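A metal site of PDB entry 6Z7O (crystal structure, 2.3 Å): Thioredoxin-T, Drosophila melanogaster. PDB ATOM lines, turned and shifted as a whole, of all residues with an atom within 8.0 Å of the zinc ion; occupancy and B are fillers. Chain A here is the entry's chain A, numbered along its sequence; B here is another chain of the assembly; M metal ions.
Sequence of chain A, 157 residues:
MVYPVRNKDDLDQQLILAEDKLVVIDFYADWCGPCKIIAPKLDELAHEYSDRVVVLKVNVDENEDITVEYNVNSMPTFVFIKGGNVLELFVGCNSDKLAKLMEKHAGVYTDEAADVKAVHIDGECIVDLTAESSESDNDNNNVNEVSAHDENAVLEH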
ATOM      1  N   LYS A   8      13.814  26.502 -13.976  1.00  0.00           N
ATOM      2  CA  LYS A   8      13.825  27.474 -15.062  1.00  0.00           C
ATOM      3  C   LYS A   8      14.689  28.690 -14.734  1.00  0.00           C
ATOM      4  O   LYS A   8      15.277  29.282 -15.651  1.00  0.00           O
ATOM      5  CB  LYS A   8      12.383  27.917 -15.357  1.00  0.00           C
ATOM      6  CG  LYS A   8      12.229  28.939 -16.468  1.00  0.00           C
ATOM      7  CD  LYS A   8      11.260  30.052 -16.050  1.00  0.00           C
ATOM      8  CE  LYS A   8      10.556  30.707 -17.249  1.00  0.00           C
ATOM      9  NZ  LYS A   8      11.491  30.957 -18.377  1.00  0.00           N
ATOM     10  N   ASP A  12      17.731  29.843 -17.063  1.00  0.00           N
ATOM     11  CA  ASP A  12      17.802  31.211 -17.586  1.00  0.00           C
ATOM     12  C   ASP A  12      19.106  31.904 -17.190  1.00  0.00           C
ATOM     13  O   ASP A  12      19.701  32.632 -18.003  1.00  0.00           O
ATOM     14  CB  ASP A  12      16.588  31.998 -17.089  1.00  0.00           C
ATOM     15  CG  ASP A  12      15.283  31.439 -17.643  1.00  0.00           C
ATOM     16  OD1 ASP A  12      15.311  30.896 -18.775  1.00  0.00           O
ATOM     17  OD2 ASP A  12      14.230  31.508 -16.945  1.00  0.00           O
ATOM     18  N   GLU A  64       8.824  19.777 -15.553  1.00  0.00           N
ATOM     19  CA  GLU A  64       7.713  19.909 -16.475  1.00  0.00           C
ATOM     20  C   GLU A  64       7.648  21.308 -17.091  1.00  0.00           C
ATOM     21  O   GLU A  64       7.244  21.452 -18.253  1.00  0.00           O
ATOM     22  CB  GLU A  64       6.408  19.557 -15.761  1.00  0.00           C
ATOM     23  CG  GLU A  64       6.504  18.237 -14.953  1.00  0.00           C
ATOM     24  CD  GLU A  64       6.805  18.445 -13.457  1.00  0.00           C
ATOM     25  OE1 GLU A  64       7.735  19.216 -13.097  1.00  0.00           O
ATOM     26  OE2 GLU A  64       6.082  17.830 -12.633  1.00  0.00           O
ATOM     27  N   ASP A  65       8.055  22.343 -16.346  1.00  0.00           N
ATOM     28  CA  ASP A  65       7.961  23.689 -16.883  1.00  0.00           C
ATOM     29  C   ASP A  65       8.928  23.899 -18.037  1.00  0.00           C
ATOM     30  O   ASP A  65       8.536  24.382 -19.110  1.00  0.00           O
ATOM     31  CB  ASP A  65       8.212  24.729 -15.793  1.00  0.00           C
ATOM     32  CG  ASP A  65       8.057  26.130 -16.329  1.00  0.00           C
ATOM     33  OD1 ASP A  65       7.191  26.301 -17.191  1.00  0.00           O
ATOM     34  OD2 ASP A  65       8.818  27.040 -15.929  1.00  0.00           O
ATOM     35  N   ILE A  66      10.197  23.536 -17.854  1.00  0.00           N
ATOM     36  CA  ILE A  66      11.172  23.717 -18.922  1.00  0.00           C
ATOM     37  C   ILE A  66      10.819  22.862 -20.137  1.00  0.00           C
ATOM     38  O   ILE A  66      11.019  23.296 -21.286  1.00  0.00           O
ATOM     39  CB  ILE A  66      12.587  23.386 -18.406  1.00  0.00           C
ATOM     40  CG1 ILE A  66      12.935  24.341 -17.260  1.00  0.00           C
ATOM     41  CG2 ILE A  66      13.576  23.481 -19.532  1.00  0.00           C
ATOM     42  CD1 ILE A  66      14.331  24.183 -16.715  1.00  0.00           C
ATOM     43  N   THR A  67      10.281  21.659 -19.919  1.00  0.00           N
ATOM     44  CA  THR A  67       9.937  20.777 -21.032  1.00  0.00           C
ATOM     45  C   THR A  67       8.814  21.373 -21.896  1.00  0.00           C
ATOM     46  O   THR A  67       8.881  21.321 -23.139  1.00  0.00           O
ATOM     47  CB  THR A  67       9.539  19.396 -20.494  1.00  0.00           C
ATOM     48  OG1 THR A  67      10.702  18.743 -19.958  1.00  0.00           O
ATOM     49  CG2 THR A  67       8.968  18.515 -21.582  1.00  0.00           C
ATOM     50  N   VAL A  68       7.815  21.973 -21.253  1.00  0.00           N
ATOM     51  CA  VAL A  68       6.706  22.584 -21.983  1.00  0.00           C
ATOM     52  C   VAL A  68       7.183  23.797 -22.779  1.00  0.00           C
ATOM     53  O   VAL A  68       6.794  23.989 -23.938  1.00  0.00           O
ATOM     54  CB  VAL A  68       5.589  22.966 -20.984  1.00  0.00           C
ATOM     55  CG1 VAL A  68       4.667  24.013 -21.586  1.00  0.00           C
ATOM     56  CG2 VAL A  68       4.837  21.745 -20.568  1.00  0.00           C
ATOM     57  N   GLU A  69       8.053  24.619 -22.176  1.00  0.00           N
ATOM     58  CA  GLU A  69       8.572  25.802 -22.841  1.00  0.00           C
ATOM     59  C   GLU A  69       9.401  25.474 -24.083  1.00  0.00           C
ATOM     60  O   GLU A  69       9.448  26.268 -25.022  1.00  0.00           O
ATOM     61  CB  GLU A  69       9.401  26.627 -21.873  1.00  0.00           C
ATOM     62  CG  GLU A  69       8.617  27.226 -20.730  1.00  0.00           C
ATOM     63  CD  GLU A  69       9.405  28.282 -19.951  1.00  0.00           C
ATOM     64  OE1 GLU A  69      10.625  28.479 -20.223  1.00  0.00           O
ATOM     65  OE2 GLU A  69       8.799  28.905 -19.064  1.00  0.00           O
ATOM     66  N   TYR A  70      10.100  24.343 -24.099  1.00  0.00           N
ATOM     67  CA  TYR A  70      10.889  23.947 -25.257  1.00  0.00           C
ATOM     68  C   TYR A  70      10.158  22.965 -26.157  1.00  0.00           C
ATOM     69  O   TYR A  70      10.761  22.436 -27.097  1.00  0.00           O
ATOM     70  CB  TYR A  70      12.236  23.376 -24.797  1.00  0.00           C
ATOM     71  CG  TYR A  70      13.182  24.481 -24.412  1.00  0.00           C
ATOM     72  CD1 TYR A  70      13.096  25.060 -23.143  1.00  0.00           C
ATOM     73  CD2 TYR A  70      14.113  24.989 -25.321  1.00  0.00           C
ATOM     74  CE1 TYR A  70      13.939  26.108 -22.772  1.00  0.00           C
ATOM     75  CE2 TYR A  70      14.967  26.050 -24.953  1.00  0.00           C
ATOM     76  CZ  TYR A  70      14.869  26.598 -23.668  1.00  0.00           C
ATOM     77  OH  TYR A  70      15.705  27.626 -23.277  1.00  0.00           O
ATOM     78  N   PHE B  80      -0.369  29.125 -14.425  1.00  0.00           N
ATOM     79  CA  PHE B  80      -0.266  28.391 -15.685  1.00  0.00           C
ATOM     80  C   PHE B  80      -0.184  26.881 -15.405  1.00  0.00           C
ATOM     81  O   PHE B  80       0.748  26.429 -14.721  1.00  0.00           O
ATOM     82  CB  PHE B  80       0.963  28.850 -16.476  1.00  0.00           C
ATOM     83  CG  PHE B  80       0.838  30.225 -17.027  1.00  0.00           C
ATOM     84  CD1 PHE B  80       0.880  31.323 -16.176  1.00  0.00           C
ATOM     85  CD2 PHE B  80       0.653  30.445 -18.379  1.00  0.00           C
ATOM     86  CE1 PHE B  80       0.757  32.601 -16.688  1.00  0.00           C
ATOM     87  CE2 PHE B  80       0.523  31.722 -18.883  1.00  0.00           C
ATOM     88  CZ  PHE B  80       0.571  32.798 -18.041  1.00  0.00           C
ATOM     89  N   LEU B  87       2.722  24.639 -13.712  1.00  0.00           N
ATOM     90  CA  LEU B  87       4.042  24.935 -14.281  1.00  0.00           C
ATOM     91  C   LEU B  87       4.671  26.181 -13.665  1.00  0.00           C
ATOM     92  O   LEU B  87       5.849  26.146 -13.258  1.00  0.00           O
ATOM     93  CB  LEU B  87       3.928  25.114 -15.798  1.00  0.00           C
ATOM     94  CG  LEU B  87       3.129  24.095 -16.586  1.00  0.00           C
ATOM     95  CD1 LEU B  87       2.982  24.572 -17.989  1.00  0.00           C
ATOM     96  CD2 LEU B  87       3.824  22.740 -16.545  1.00  0.00           C
ATOM     97  N   GLU B  88       3.918  27.287 -13.592  1.00  0.00           N
ATOM     98  CA  GLU B  88       4.436  28.599 -13.261  1.00  0.00           C
ATOM     99  C   GLU B  88       3.346  29.456 -12.638  1.00  0.00           C
ATOM    100  O   GLU B  88       2.169  29.356 -12.982  1.00  0.00           O
ATOM    101  CB  GLU B  88       4.968  29.311 -14.493  1.00  0.00           C
ATOM    102  CG  GLU B  88       6.394  29.761 -14.358  1.00  0.00           C
ATOM    103  CD  GLU B  88       6.874  30.502 -15.582  1.00  0.00           C
ATOM    104  OE1 GLU B  88       7.035  31.739 -15.533  1.00  0.00           O
ATOM    105  OE2 GLU B  88       7.060  29.810 -16.605  1.00  0.00           O
ATOM    106  N   LEU B  89       3.773  30.341 -11.745  1.00  0.00           N
ATOM    107  CA  LEU B  89       2.890  31.269 -11.055  1.00  0.00           C
ATOM    108  C   LEU B  89       3.380  32.683 -11.363  1.00  0.00           C
ATOM    109  O   LEU B  89       4.589  32.932 -11.415  1.00  0.00           O
ATOM    110  CB  LEU B  89       2.892  30.988  -9.547  1.00  0.00           C
ATOM    111  CG  LEU B  89       1.702  31.567  -8.793  1.00  0.00           C
ATOM    112  CD1 LEU B  89       0.646  30.504  -8.698  1.00  0.00           C
ATOM    113  CD2 LEU B  89       2.015  32.099  -7.437  1.00  0.00           C
ATOM    114  N   LEU B 101       4.266  34.888 -21.675  1.00  0.00           N
ATOM    115  CA  LEU B 101       4.140  33.615 -20.956  1.00  0.00           C
ATOM    116  C   LEU B 101       3.115  32.700 -21.606  1.00  0.00           C
ATOM    117  O   LEU B 101       3.333  31.491 -21.719  1.00  0.00           O
ATOM    118  CB  LEU B 101       3.762  33.862 -19.488  1.00  0.00           C
ATOM    119  CG  LEU B 101       4.897  34.396 -18.605  1.00  0.00           C
ATOM    120  CD1 LEU B 101       4.341  34.693 -17.227  1.00  0.00           C
ATOM    121  CD2 LEU B 101       6.074  33.429 -18.523  1.00  0.00           C
ATOM    122  N   LYS B 104       4.869  31.135 -24.744  1.00  0.00           N
ATOM    123  CA  LYS B 104       5.920  30.165 -24.427  1.00  0.00           C
ATOM    124  C   LYS B 104       5.380  28.825 -23.933  1.00  0.00           C
ATOM    125  O   LYS B 104       6.123  27.842 -23.972  1.00  0.00           O
ATOM    126  CB  LYS B 104       6.860  30.721 -23.341  1.00  0.00           C
ATOM    127  CG  LYS B 104       8.089  31.442 -23.856  1.00  0.00           C
ATOM    128  CD  LYS B 104       9.099  31.772 -22.729  1.00  0.00           C
ATOM    129  CE  LYS B 104       8.432  32.504 -21.584  1.00  0.00           C
ATOM    130  NZ  LYS B 104       8.917  32.004 -20.268  1.00  0.00           N
ATOM    131  N   HIS B 105       4.148  28.768 -23.426  1.00  0.00           N
ATOM    132  CA  HIS B 105       3.601  27.564 -22.813  1.00  0.00           C
ATOM    133  C   HIS B 105       2.434  26.985 -23.620  1.00  0.00           C
ATOM    134  O   HIS B 105       1.776  26.068 -23.137  1.00  0.00           O
ATOM    135  CB  HIS B 105       3.144  27.843 -21.374  1.00  0.00           C
ATOM    136  CG  HIS B 105       4.252  28.208 -20.440  1.00  0.00           C
ATOM    137  ND1 HIS B 105       4.620  29.525 -20.203  1.00  0.00           N
ATOM    138  CD2 HIS B 105       5.074  27.450 -19.676  1.00  0.00           C
ATOM    139  CE1 HIS B 105       5.621  29.550 -19.334  1.00  0.00           C
ATOM    140  NE2 HIS B 105       5.910  28.314 -18.996  1.00  0.00           N
HETATM  141 ZN    ZN M   1       7.384  28.304 -17.826  1.00  0.00          ZN
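A ring nitrogen (ND1) of His 105 of chain B is in hydrogen-bond range of the backbone carbonyl oxygen of Leu 101 of chain B (2.8 Å).
The side-chain amino group (NZ) of Lys 104 of chain B lies within salt-bridge range of the side-chain carboxylate (OE1) of Glu 69 (3.9 Å).
The side-chain amino group (NZ) of Lys 8 lies within salt-bridge range of the side-chain carboxylate (OE1) of Glu 69, 3.2 Å away.
O of Glu 88 of chain B lies within hydrogen-bond range of N of Phe 80 of chain B (2.9 Å).
The zinc ion is bound by NE2 of His 105 of chain B (1.9 Å), OE2 of Glu 88 of chain B (2.0 Å), OE2 of Glu 69 (2.0 Å) and OD1 of Asp 65 (2.1 Å).
Slightly farther from the zinc ion lies the side-chain carboxylate (OD2) of Asp 65 (2.7 Å).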
